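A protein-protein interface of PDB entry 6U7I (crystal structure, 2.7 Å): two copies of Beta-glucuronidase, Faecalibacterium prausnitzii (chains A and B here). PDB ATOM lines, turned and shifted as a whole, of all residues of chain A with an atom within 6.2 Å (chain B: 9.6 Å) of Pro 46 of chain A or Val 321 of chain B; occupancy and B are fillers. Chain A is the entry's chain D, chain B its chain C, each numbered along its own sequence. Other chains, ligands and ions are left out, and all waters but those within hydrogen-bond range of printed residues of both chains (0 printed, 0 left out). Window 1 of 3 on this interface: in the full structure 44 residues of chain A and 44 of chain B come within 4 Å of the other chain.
Of chain B, only Val 321 comes within 4 Å of Pro 46 of chain A. Val 321 of chain B touches just these residues of chain A: Ala 44 (3.6 Å), Pro 46 (3.98 Å), Ala 47 (3.6 Å), Ala 313 (3.2 Å) and His 314 (3.7 Å). No residue of chain B comes within 4 Å of Val 45 of chain A. Of chain B, only Val 321 (3.6 Å) comes within 4 Å of Ala 47 of chain A. Of the printed residues of chain B, His 314 of chain A touches His 314 (3.6 Å), Asp 319 (2.7 Å) and Val 321 (3.7 Å). Of the printed residues of chain B, Ala 313 of chain A touches Val 321. Printed residues of chain A within 4 Å of His 314 of chain B: His 314. Of the printed residues of chain A, Pro 320 of chain B touches Ala 44 (3.9 Å). Printed residues of chain A within 4 Å of Asp 319 of chain B: His 314 (2.7 Å). Printed residues of chain A within 4 Å of Val 324 of chain B: Gln 52. The nearest residue of chain B that does not touch Pro 46 of chain A is Pro 320 of chain B (6.3 Å). The nearest printed residue of chain B that does not touch Ala 313 of chain A is Leu 322 of chain B (4.1 Å).
His 314 of chain A touches its own counterpart, His 314 of chain B. Of the 13 pairs that touch across the chains among the printed residues, 1 has its exchanged pair printed and touching as well.
The side-chain amino group (NZ) of Lys 325 of chain B lies close to the backbone carbonyl oxygen (O) of Asp 51 of chain A. The side-chain carboxylate of Asp 319 of chain B is in hydrogen-bond range of a ring nitrogen (NE2) of His 314 of chain A (2.7 Å). O of Gln 52 of chain A sits at hydrogen-bond distance from ND2 of Asn 328 of chain B, 2.5 Å away.
Among the printed residues, pairs that only touch across the chains: Ala 313 of chain A with Val 321 of chain B (3.2 Å), Gln 52 of chain A with Val 324 of chain B (3.2 Å), Ala 44 of chain A with Val 321 of chain B (3.6 Å), His 314 of chain A with His 314 of chain B (3.6 Å), Ala 47 of chain A with Val 321 of chain B (3.6 Å), His 314 of chain A with Val 321 of chain B (3.7 Å), Thr 312 of chain A with Phe 311 of chain B (3.7 Å), Gln 52 of chain A with Lys 325 of chain B (3.7 Å), Ala 44 of chain A with Pro 320 of chain B (3.9 Å) and Pro 46 of chain A with Val 321 of chain B (3.98 Å).
NE2 of Gln 52 of chain A lies within hydrogen-bond range of O of Ser 48 of chain A, 2.9 Å away. The backbone carbonyl oxygen of Val 324 of chain B lies within hydrogen-bond range of the side-chain amide nitrogen of Asn 328 of chain B. A ring nitrogen (NE2) of His 314 of chain B is in hydrogen-bond range of the side-chain carboxylate (OD2) of Asp 319 of chain B (3.1 Å). The side-chain carboxylate of Asp 319 of chain B lies within hydrogen-bond range of the backbone NH of Val 321 of chain B (3.1 Å). The backbone NH of Ala 44 of chain A lies within hydrogen-bond range of the side-chain amide oxygen of Gln 52 of chain A. OD1 of Asp 319 of chain B lies within hydrogen-bond range of N of Leu 322 of chain B.
Printed residues of chain A that touch a printed residue of chain B: Ala 44, Pro 46, Ala 47, Asp 51, Gln 52, Thr 312, Ala 313 and His 314. Hydrophobic or aromatic side chains of chain A that line the printed part of chain B: Ala 44, Ala 47, Ala 313 and His 314. Along chain A the printed residues that touch a printed residue of chain B span positions 44 to 314. Among the printed residues, 13 pairs touch across the chains.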
ATOM      1  N   ASP A  16     -29.356   4.896  17.065  1.00  0.00           N
ATOM      2  CA  ASP A  16     -28.144   4.402  17.713  1.00  0.00           C
ATOM      3  C   ASP A  16     -28.490   3.239  18.644  1.00  0.00           C
ATOM      4  O   ASP A  16     -29.642   3.002  18.998  1.00  0.00           O
ATOM      5  CB  ASP A  16     -27.451   5.516  18.498  1.00  0.00           C
ATOM      6  CG  ASP A  16     -27.018   6.686  17.603  1.00  0.00           C
ATOM      7  OD1 ASP A  16     -26.659   6.460  16.413  1.00  0.00           O
ATOM      8  OD2 ASP A  16     -27.031   7.840  18.103  1.00  0.00           O
ATOM      9  N   GLY A  17     -27.468   2.504  19.051  1.00  0.00           N
ATOM     10  CA  GLY A  17     -27.658   1.316  19.850  1.00  0.00           C
ATOM     11  C   GLY A  17     -26.835   0.172  19.314  1.00  0.00           C
ATOM     12  O   GLY A  17     -26.030   0.326  18.394  1.00  0.00           O
ATOM     13  N   ALA A  44     -21.633  -2.116  18.707  1.00  0.00           N
ATOM     14  CA  ALA A  44     -22.135  -0.816  19.143  1.00  0.00           C
ATOM     15  C   ALA A  44     -22.106   0.207  18.004  1.00  0.00           C
ATOM     16  O   ALA A  44     -21.077   0.373  17.335  1.00  0.00           O
ATOM     17  CB  ALA A  44     -21.317  -0.312  20.329  1.00  0.00           C
ATOM     18  N   VAL A  45     -23.236   0.888  17.792  1.00  0.00           N
ATOM     19  CA  VAL A  45     -23.384   1.959  16.797  1.00  0.00           C
ATOM     20  C   VAL A  45     -23.949   3.209  17.472  1.00  0.00           C
ATOM     21  O   VAL A  45     -24.877   3.104  18.292  1.00  0.00           O
ATOM     22  CB  VAL A  45     -24.281   1.532  15.624  1.00  0.00           C
ATOM     23  CG1 VAL A  45     -24.220   2.557  14.501  1.00  0.00           C
ATOM     24  CG2 VAL A  45     -23.897   0.161  15.101  1.00  0.00           C
ATOM     25  N   PRO A  46     -23.394   4.408  17.205  1.00  0.00           N
ATOM     26  CA  PRO A  46     -22.198   4.630  16.380  1.00  0.00           C
ATOM     27  C   PRO A  46     -20.862   4.322  17.115  1.00  0.00           C
ATOM     28  O   PRO A  46     -20.798   4.451  18.341  1.00  0.00           O
ATOM     29  CB  PRO A  46     -22.299   6.112  16.042  1.00  0.00           C
ATOM     30  CG  PRO A  46     -22.888   6.694  17.271  1.00  0.00           C
ATOM     31  CD  PRO A  46     -23.857   5.660  17.821  1.00  0.00           C
ATOM     32  N   ALA A  47     -19.849   3.908  16.342  1.00  0.00           N
ATOM     33  CA  ALA A  47     -18.462   3.677  16.731  1.00  0.00           C
ATOM     34  C   ALA A  47     -17.810   2.943  15.587  1.00  0.00           C
ATOM     35  O   ALA A  47     -18.523   2.448  14.712  1.00  0.00           O
ATOM     36  CB  ALA A  47     -18.306   2.825  17.988  1.00  0.00           C
ATOM     37  N   SER A  48     -16.480   2.854  15.574  1.00  0.00           N
ATOM     38  CA  SER A  48     -15.837   1.941  14.645  1.00  0.00           C
ATOM     39  C   SER A  48     -16.112   0.523  15.107  1.00  0.00           C
ATOM     40  O   SER A  48     -16.328   0.268  16.297  1.00  0.00           O
ATOM     41  CB  SER A  48     -14.324   2.164  14.591  1.00  0.00           C
ATOM     42  OG  SER A  48     -13.988   3.531  14.449  1.00  0.00           O
ATOM     43  N   ASP A  51     -12.338  -2.211  16.918  1.00  0.00           N
ATOM     44  CA  ASP A  51     -11.800  -2.487  18.251  1.00  0.00           C
ATOM     45  C   ASP A  51     -12.832  -3.081  19.201  1.00  0.00           C
ATOM     46  O   ASP A  51     -12.781  -2.834  20.404  1.00  0.00           O
ATOM     47  CB  ASP A  51     -11.213  -1.228  18.883  1.00  0.00           C
ATOM     48  CG  ASP A  51      -9.986  -0.720  18.151  1.00  0.00           C
ATOM     49  OD1 ASP A  51      -9.557  -1.347  17.146  1.00  0.00           O
ATOM     50  OD2 ASP A  51      -9.468   0.335  18.580  1.00  0.00           O
ATOM     51  N   GLN A  52     -13.766  -3.869  18.692  1.00  0.00           N
ATOM     52  CA  GLN A  52     -14.917  -4.247  19.487  1.00  0.00           C
ATOM     53  C   GLN A  52     -15.045  -5.743  19.737  1.00  0.00           C
ATOM     54  O   GLN A  52     -15.867  -6.137  20.569  1.00  0.00           O
ATOM     55  CB  GLN A  52     -16.199  -3.733  18.820  1.00  0.00           C
ATOM     56  CG  GLN A  52     -16.536  -2.270  19.086  1.00  0.00           C
ATOM     57  CD  GLN A  52     -18.006  -1.973  18.789  1.00  0.00           C
ATOM     58  OE1 GLN A  52     -18.876  -2.683  19.264  1.00  0.00           O
ATOM     59  NE2 GLN A  52     -18.282  -0.939  17.986  1.00  0.00           N
ATOM     60  N   ILE A 187     -20.142   2.418  10.967  1.00  0.00           N
ATOM     61  CA  ILE A 187     -21.055   3.551  11.096  1.00  0.00           C
ATOM     62  C   ILE A 187     -20.601   4.436  12.252  1.00  0.00           C
ATOM     63  O   ILE A 187     -20.872   4.138  13.418  1.00  0.00           O
ATOM     64  CB  ILE A 187     -22.505   3.080  11.278  1.00  0.00           C
ATOM     65  CG1 ILE A 187     -22.789   1.907  10.342  1.00  0.00           C
ATOM     66  CG2 ILE A 187     -23.445   4.214  10.968  1.00  0.00           C
ATOM     67  CD1 ILE A 187     -24.075   1.149  10.642  1.00  0.00           C
ATOM     68  N   HIS A 188     -19.906   5.539  11.935  1.00  0.00           N
ATOM     69  CA  HIS A 188     -19.184   6.306  12.950  1.00  0.00           C
ATOM     70  C   HIS A 188     -19.996   7.417  13.580  1.00  0.00           C
ATOM     71  O   HIS A 188     -19.634   7.873  14.676  1.00  0.00           O
ATOM     72  CB  HIS A 188     -17.935   6.977  12.379  1.00  0.00           C
ATOM     73  CG  HIS A 188     -16.852   6.032  11.994  1.00  0.00           C
ATOM     74  ND1 HIS A 188     -16.164   6.150  10.805  1.00  0.00           N
ATOM     75  CD2 HIS A 188     -16.333   4.959  12.631  1.00  0.00           C
ATOM     76  CE1 HIS A 188     -15.261   5.190  10.730  1.00  0.00           C
ATOM     77  NE2 HIS A 188     -15.350   4.448  11.818  1.00  0.00           N
ATOM     78  N   ARG A 189     -21.028   7.912  12.904  1.00  0.00           N
ATOM     79  CA  ARG A 189     -21.758   9.072  13.388  1.00  0.00           C
ATOM     80  C   ARG A 189     -23.191   8.682  13.701  1.00  0.00           C
ATOM     81  O   ARG A 189     -23.680   7.656  13.207  1.00  0.00           O
ATOM     82  CB  ARG A 189     -21.721  10.205  12.355  1.00  0.00           C
ATOM     83  CG  ARG A 189     -20.525  11.096  12.463  1.00  0.00           C
ATOM     84  CD  ARG A 189     -19.990  11.494  11.108  1.00  0.00           C
ATOM     85  NE  ARG A 189     -18.639  12.031  11.224  1.00  0.00           N
ATOM     86  CZ  ARG A 189     -18.074  12.855  10.352  1.00  0.00           C
ATOM     87  NH1 ARG A 189     -18.738  13.262   9.279  1.00  0.00           N
ATOM     88  NH2 ARG A 189     -16.838  13.281  10.560  1.00  0.00           N
ATOM     89  N   PRO A 190     -23.895   9.469  14.530  1.00  0.00           N
ATOM     90  CA  PRO A 190     -25.260   9.079  14.934  1.00  0.00           C
ATOM     91  C   PRO A 190     -26.187   8.890  13.738  1.00  0.00           C
ATOM     92  O   PRO A 190     -26.164   9.663  12.779  1.00  0.00           O
ATOM     93  CB  PRO A 190     -25.717  10.236  15.826  1.00  0.00           C
ATOM     94  CG  PRO A 190     -24.446  10.839  16.354  1.00  0.00           C
ATOM     95  CD  PRO A 190     -23.441  10.684  15.229  1.00  0.00           C
ATOM     96  N   VAL A 191     -26.970   7.813  13.798  1.00  0.00           N
ATOM     97  CA  VAL A 191     -27.935   7.439  12.767  1.00  0.00           C
ATOM     98  C   VAL A 191     -29.315   7.895  13.208  1.00  0.00           C
ATOM     99  O   VAL A 191     -29.809   7.461  14.256  1.00  0.00           O
ATOM    100  CB  VAL A 191     -27.933   5.927  12.525  1.00  0.00           C
ATOM    101  CG1 VAL A 191     -29.031   5.554  11.555  1.00  0.00           C
ATOM    102  CG2 VAL A 191     -26.581   5.498  12.015  1.00  0.00           C
ATOM    103  N   THR A 312      -9.928   5.303  22.452  1.00  0.00           N
ATOM    104  CA  THR A 312     -10.058   3.923  22.889  1.00  0.00           C
ATOM    105  C   THR A 312     -11.499   3.447  22.712  1.00  0.00           C
ATOM    106  O   THR A 312     -12.448   4.165  23.051  1.00  0.00           O
ATOM    107  CB  THR A 312      -9.611   3.840  24.355  1.00  0.00           C
ATOM    108  OG1 THR A 312      -8.260   4.316  24.459  1.00  0.00           O
ATOM    109  CG2 THR A 312      -9.739   2.412  24.943  1.00  0.00           C
ATOM    110  N   ALA A 313     -11.652   2.239  22.150  1.00  0.00           N
ATOM    111  CA  ALA A 313     -12.941   1.571  21.897  1.00  0.00           C
ATOM    112  C   ALA A 313     -13.762   2.246  20.803  1.00  0.00           C
ATOM    113  O   ALA A 313     -14.289   1.581  19.910  1.00  0.00           O
ATOM    114  CB  ALA A 313     -13.772   1.485  23.171  1.00  0.00           C
ATOM    115  N   HIS A 314     -13.866   3.567  20.853  1.00  0.00           N
ATOM    116  CA  HIS A 314     -14.676   4.281  19.893  1.00  0.00           C
ATOM    117  C   HIS A 314     -14.048   4.310  18.510  1.00  0.00           C
ATOM    118  O   HIS A 314     -14.775   4.416  17.516  1.00  0.00           O
ATOM    119  CB  HIS A 314     -14.943   5.674  20.441  1.00  0.00           C
ATOM    120  CG  HIS A 314     -15.812   5.656  21.663  1.00  0.00           C
ATOM    121  ND1 HIS A 314     -17.188   5.681  21.606  1.00  0.00           N
ATOM    122  CD2 HIS A 314     -15.501   5.543  22.975  1.00  0.00           C
ATOM    123  CE1 HIS A 314     -17.685   5.614  22.825  1.00  0.00           C
ATOM    124  NE2 HIS A 314     -16.685   5.529  23.678  1.00  0.00           N
ATOM    125  N   GLY A 315     -12.734   4.167  18.414  1.00  0.00           N
ATOM    126  CA  GLY A 315     -12.069   4.251  17.116  1.00  0.00           C
ATOM    127  C   GLY A 315     -12.195   5.650  16.551  1.00  0.00           C
ATOM    128  O   GLY A 315     -11.884   6.637  17.222  1.00  0.00           O
ATOM    129  N   GLY A 317     -15.219   6.501  15.778  1.00  0.00           N
ATOM    130  CA  GLY A 317     -16.561   6.826  16.193  1.00  0.00           C
ATOM    131  C   GLY A 317     -16.644   8.156  16.919  1.00  0.00           C
ATOM    132  O   GLY A 317     -15.663   8.727  17.398  1.00  0.00           O
ATOM    133  N   PHE A 318     -17.870   8.640  17.008  1.00  0.00           N
ATOM    134  CA  PHE A 318     -18.158   9.937  17.582  1.00  0.00           C
ATOM    135  C   PHE A 318     -18.408   9.765  19.076  1.00  0.00           C
ATOM    136  O   PHE A 318     -19.067   8.806  19.496  1.00  0.00           O
ATOM    137  CB  PHE A 318     -19.370  10.531  16.856  1.00  0.00           C
ATOM    138  CG  PHE A 318     -19.997  11.671  17.568  1.00  0.00           C
ATOM    139  CD1 PHE A 318     -19.351  12.898  17.622  1.00  0.00           C
ATOM    140  CD2 PHE A 318     -21.217  11.517  18.201  1.00  0.00           C
ATOM    141  CE1 PHE A 318     -19.917  13.955  18.296  1.00  0.00           C
ATOM    142  CE2 PHE A 318     -21.790  12.567  18.873  1.00  0.00           C
ATOM    143  CZ  PHE A 318     -21.142  13.789  18.922  1.00  0.00           C
ATOM    144  N   PHE B 311     -14.369   4.553  33.160  1.00  0.00           N
ATOM    145  CA  PHE B 311     -13.639   4.725  31.911  1.00  0.00           C
ATOM    146  C   PHE B 311     -13.223   6.186  31.775  1.00  0.00           C
ATOM    147  O   PHE B 311     -13.860   7.081  32.334  1.00  0.00           O
ATOM    148  CB  PHE B 311     -14.475   4.297  30.703  1.00  0.00           C
ATOM    149  CG  PHE B 311     -13.701   4.258  29.408  1.00  0.00           C
ATOM    150  CD1 PHE B 311     -12.651   3.377  29.241  1.00  0.00           C
ATOM    151  CD2 PHE B 311     -14.045   5.090  28.350  1.00  0.00           C
ATOM    152  CE1 PHE B 311     -11.951   3.332  28.043  1.00  0.00           C
ATOM    153  CE2 PHE B 311     -13.344   5.050  27.155  1.00  0.00           C
ATOM    154  CZ  PHE B 311     -12.306   4.169  26.994  1.00  0.00           C
ATOM    155  N   HIS B 314     -15.673   9.222  30.343  1.00  0.00           N
ATOM    156  CA  HIS B 314     -17.036   8.813  30.634  1.00  0.00           C
ATOM    157  C   HIS B 314     -17.269   8.637  32.130  1.00  0.00           C
ATOM    158  O   HIS B 314     -18.432   8.685  32.583  1.00  0.00           O
ATOM    159  CB  HIS B 314     -17.347   7.513  29.895  1.00  0.00           C
ATOM    160  CG  HIS B 314     -17.613   7.701  28.435  1.00  0.00           C
ATOM    161  ND1 HIS B 314     -18.866   7.966  27.934  1.00  0.00           N
ATOM    162  CD2 HIS B 314     -16.783   7.650  27.366  1.00  0.00           C
ATOM    163  CE1 HIS B 314     -18.797   8.082  26.620  1.00  0.00           C
ATOM    164  NE2 HIS B 314     -17.543   7.897  26.249  1.00  0.00           N
ATOM    165  N   GLY B 317     -20.287   6.998  33.702  1.00  0.00           N
ATOM    166  CA  GLY B 317     -21.323   7.068  32.714  1.00  0.00           C
ATOM    167  C   GLY B 317     -21.338   5.850  31.815  1.00  0.00           C
ATOM    168  O   GLY B 317     -20.359   5.107  31.681  1.00  0.00           O
ATOM    169  N   PHE B 318     -22.483   5.678  31.167  1.00  0.00           N
ATOM    170  CA  PHE B 318     -22.741   4.511  30.354  1.00  0.00           C
ATOM    171  C   PHE B 318     -21.982   4.633  29.041  1.00  0.00           C
ATOM    172  O   PHE B 318     -21.729   5.743  28.548  1.00  0.00           O
ATOM    173  CB  PHE B 318     -24.255   4.385  30.138  1.00  0.00           C
ATOM    174  CG  PHE B 318     -24.644   3.335  29.160  1.00  0.00           C
ATOM    175  CD1 PHE B 318     -24.334   2.006  29.391  1.00  0.00           C
ATOM    176  CD2 PHE B 318     -25.304   3.678  28.004  1.00  0.00           C
ATOM    177  CE1 PHE B 318     -24.680   1.032  28.467  1.00  0.00           C
ATOM    178  CE2 PHE B 318     -25.661   2.713  27.080  1.00  0.00           C
ATOM    179  CZ  PHE B 318     -25.348   1.388  27.310  1.00  0.00           C
ATOM    180  N   ASP B 319     -21.596   3.474  28.487  1.00  0.00           N
ATOM    181  CA  ASP B 319     -20.870   3.404  27.218  1.00  0.00           C
ATOM    182  C   ASP B 319     -21.132   2.053  26.552  1.00  0.00           C
ATOM    183  O   ASP B 319     -20.587   1.022  26.972  1.00  0.00           O
ATOM    184  CB  ASP B 319     -19.355   3.621  27.440  1.00  0.00           C
ATOM    185  CG  ASP B 319     -18.572   3.781  26.141  1.00  0.00           C
ATOM    186  OD1 ASP B 319     -18.512   2.816  25.360  1.00  0.00           O
ATOM    187  OD2 ASP B 319     -17.997   4.867  25.908  1.00  0.00           O
ATOM    188  N   PRO B 320     -21.979   2.003  25.527  1.00  0.00           N
ATOM    189  CA  PRO B 320     -22.246   0.708  24.884  1.00  0.00           C
ATOM    190  C   PRO B 320     -21.035   0.120  24.167  1.00  0.00           C
ATOM    191  O   PRO B 320     -20.878  -1.112  24.172  1.00  0.00           O
ATOM    192  CB  PRO B 320     -23.394   1.025  23.914  1.00  0.00           C
ATOM    193  CG  PRO B 320     -23.375   2.511  23.752  1.00  0.00           C
ATOM    194  CD  PRO B 320     -22.838   3.079  25.011  1.00  0.00           C
ATOM    195  N   VAL B 321     -20.181   0.970  23.564  1.00  0.00           N
ATOM    196  CA  VAL B 321     -18.952   0.517  22.897  1.00  0.00           C
ATOM    197  C   VAL B 321     -18.026  -0.164  23.891  1.00  0.00           C
ATOM    198  O   VAL B 321     -17.492  -1.250  23.634  1.00  0.00           O
ATOM    199  CB  VAL B 321     -18.234   1.698  22.217  1.00  0.00           C
ATOM    200  CG1 VAL B 321     -17.167   1.184  21.290  1.00  0.00           C
ATOM    201  CG2 VAL B 321     -19.223   2.562  21.469  1.00  0.00           C
ATOM    202  N   LEU B 322     -17.811   0.478  25.042  1.00  0.00           N
ATOM    203  CA  LEU B 322     -17.054  -0.172  26.100  1.00  0.00           C
ATOM    204  C   LEU B 322     -17.687  -1.502  26.483  1.00  0.00           C
ATOM    205  O   LEU B 322     -16.981  -2.499  26.670  1.00  0.00           O
ATOM    206  CB  LEU B 322     -16.929   0.747  27.313  1.00  0.00           C
ATOM    207  CG  LEU B 322     -15.632   0.356  28.030  1.00  0.00           C
ATOM    208  CD1 LEU B 322     -14.436   0.678  27.155  1.00  0.00           C
ATOM    209  CD2 LEU B 322     -15.501   0.990  29.407  1.00  0.00           C
ATOM    210  N   ASN B 323     -19.019  -1.553  26.547  1.00  0.00           N
ATOM    211  CA  ASN B 323     -19.696  -2.770  26.976  1.00  0.00           C
ATOM    212  C   ASN B 323     -19.431  -3.927  26.023  1.00  0.00           C
ATOM    213  O   ASN B 323     -19.105  -5.042  26.453  1.00  0.00           O
ATOM    214  CB  ASN B 323     -21.179  -2.502  27.089  1.00  0.00           C
ATOM    215  CG  ASN B 323     -21.559  -1.983  28.440  1.00  0.00           C
ATOM    216  OD1 ASN B 323     -20.761  -1.325  29.119  1.00  0.00           O
ATOM    217  ND2 ASN B 323     -22.796  -2.258  28.845  1.00  0.00           N
ATOM    218  N   VAL B 324     -19.574  -3.689  24.721  1.00  0.00           N
ATOM    219  CA  VAL B 324     -19.274  -4.734  23.744  1.00  0.00           C
ATOM    220  C   VAL B 324     -17.800  -5.147  23.826  1.00  0.00           C
ATOM    221  O   VAL B 324     -17.476  -6.341  23.854  1.00  0.00           O
ATOM    222  CB  VAL B 324     -19.662  -4.273  22.325  1.00  0.00           C
ATOM    223  CG1 VAL B 324     -19.066  -5.198  21.268  1.00  0.00           C
ATOM    224  CG2 VAL B 324     -21.173  -4.200  22.167  1.00  0.00           C
ATOM    225  N   LYS B 325     -16.881  -4.174  23.857  1.00  0.00           N
ATOM    226  CA  LYS B 325     -15.459  -4.523  23.923  1.00  0.00           C
ATOM    227  C   LYS B 325     -15.167  -5.380  25.145  1.00  0.00           C
ATOM    228  O   LYS B 325     -14.564  -6.455  25.034  1.00  0.00           O
ATOM    229  CB  LYS B 325     -14.590  -3.264  23.944  1.00  0.00           C
ATOM    230  CG  LYS B 325     -13.162  -3.575  24.224  1.00  0.00           C
ATOM    231  CD  LYS B 325     -12.240  -2.498  23.737  1.00  0.00           C
ATOM    232  CE  LYS B 325     -10.979  -3.133  23.184  1.00  0.00           C
ATOM    233  NZ  LYS B 325     -10.105  -2.134  22.532  1.00  0.00           N
ATOM    234  N   ASP B 326     -15.640  -4.928  26.313  1.00  0.00           N
ATOM    235  CA  ASP B 326     -15.426  -5.632  27.574  1.00  0.00           C
ATOM    236  C   ASP B 326     -15.960  -7.063  27.539  1.00  0.00           C
ATOM    237  O   ASP B 326     -15.274  -7.985  27.989  1.00  0.00           O
ATOM    238  CB  ASP B 326     -16.080  -4.852  28.716  1.00  0.00           C
ATOM    239  CG  ASP B 326     -15.290  -3.608  29.119  1.00  0.00           C
ATOM    240  OD1 ASP B 326     -14.437  -3.152  28.325  1.00  0.00           O
ATOM    241  OD2 ASP B 326     -15.525  -3.085  30.241  1.00  0.00           O
ATOM    242  N   VAL B 327     -17.179  -7.281  27.024  1.00  0.00           N
ATOM    243  CA  VAL B 327     -17.729  -8.640  27.042  1.00  0.00           C
ATOM    244  C   VAL B 327     -16.899  -9.557  26.160  1.00  0.00           C
ATOM    245  O   VAL B 327     -16.690 -10.735  26.476  1.00  0.00           O
ATOM    246  CB  VAL B 327     -19.210  -8.656  26.618  1.00  0.00           C
ATOM    247  CG1 VAL B 327     -19.593 -10.028  26.104  1.00  0.00           C
ATOM    248  CG2 VAL B 327     -20.073  -8.322  27.797  1.00  0.00           C
ATOM    249  N   ASN B 328     -16.405  -9.035  25.051  1.00  0.00           N
ATOM    250  CA  ASN B 328     -15.630  -9.866  24.145  1.00  0.00           C
ATOM    251  C   ASN B 328     -14.296 -10.267  24.742  1.00  0.00           C
ATOM    252  O   ASN B 328     -13.802 -11.362  24.445  1.00  0.00           O
ATOM    253  CB  ASN B 328     -15.427  -9.136  22.835  1.00  0.00           C
ATOM    254  CG  ASN B 328     -16.634  -9.240  21.955  1.00  0.00           C
ATOM    255  OD1 ASN B 328     -17.192 -10.322  21.802  1.00  0.00           O
ATOM    256  ND2 ASN B 328     -17.065  -8.118  21.391  1.00  0.00           N
ATOM    257  N   LEU B 329     -13.704  -9.405  25.576  1.00  0.00           N
ATOM    258  CA  LEU B 329     -12.473  -9.768  26.279  1.00  0.00           C
ATOM    259  C   LEU B 329     -12.730 -10.784  27.380  1.00  0.00           C
ATOM    260  O   LEU B 329     -11.805 -11.513  27.770  1.00  0.00           O
ATOM    261  CB  LEU B 329     -11.821  -8.537  26.898  1.00  0.00           C
ATOM    262  CG  LEU B 329     -11.268  -7.477  25.965  1.00  0.00           C
ATOM    263  CD1 LEU B 329     -11.119  -6.185  26.761  1.00  0.00           C
ATOM    264  CD2 LEU B 329      -9.935  -7.961  25.411  1.00  0.00           C
ATOM    265  N   GLU B 348     -28.606  -2.015  30.013  1.00  0.00           N
ATOM    266  CA  GLU B 348     -28.030  -2.543  28.786  1.00  0.00           C
ATOM    267  C   GLU B 348     -26.886  -3.520  29.028  1.00  0.00           C
ATOM    268  O   GLU B 348     -26.595  -4.344  28.155  1.00  0.00           O
ATOM    269  CB  GLU B 348     -27.570  -1.370  27.923  1.00  0.00           C
ATOM    270  CG  GLU B 348     -28.731  -0.552  27.314  1.00  0.00           C
ATOM    271  CD  GLU B 348     -29.097   0.697  28.129  1.00  0.00           C
ATOM    272  OE1 GLU B 348     -29.181   0.614  29.394  1.00  0.00           O
ATOM    273  OE2 GLU B 348     -29.293   1.763  27.485  1.00  0.00           O
ATOM    274  N   LEU B 352     -26.768  -7.375  27.327  1.00  0.00           N
ATOM    275  CA  LEU B 352     -25.658  -7.901  26.564  1.00  0.00           C
ATOM    276  C   LEU B 352     -25.236  -9.264  27.098  1.00  0.00           C
ATOM    277  O   LEU B 352     -24.994 -10.186  26.307  1.00  0.00           O
ATOM    278  CB  LEU B 352     -24.517  -6.893  26.553  1.00  0.00           C
ATOM    279  CG  LEU B 352     -23.385  -7.235  25.586  1.00  0.00           C
ATOM    280  CD1 LEU B 352     -23.855  -7.277  24.138  1.00  0.00           C
ATOM    281  CD2 LEU B 352     -22.281  -6.223  25.749  1.00  0.00           C
ATOM    282  N   ARG B 575      -8.134  -1.147  28.752  1.00  0.00           N
ATOM    283  CA  ARG B 575      -8.516  -2.508  28.405  1.00  0.00           C
ATOM    284  C   ARG B 575      -7.400  -3.216  27.650  1.00  0.00           C
ATOM    285  O   ARG B 575      -7.634  -3.885  26.642  1.00  0.00           O
ATOM    286  CB  ARG B 575      -9.817  -2.513  27.599  1.00  0.00           C
ATOM    287  CG  ARG B 575     -11.073  -2.595  28.442  1.00  0.00           C
ATOM    288  CD  ARG B 575     -11.213  -1.418  29.364  1.00  0.00           C
ATOM    289  NE  ARG B 575     -12.444  -1.569  30.120  1.00  0.00           N
ATOM    290  CZ  ARG B 575     -12.747  -0.900  31.220  1.00  0.00           C
ATOM    291  NH1 ARG B 575     -11.914   0.002  31.712  1.00  0.00           N
ATOM    292  NH2 ARG B 575     -13.906  -1.137  31.815  1.00  0.00           N
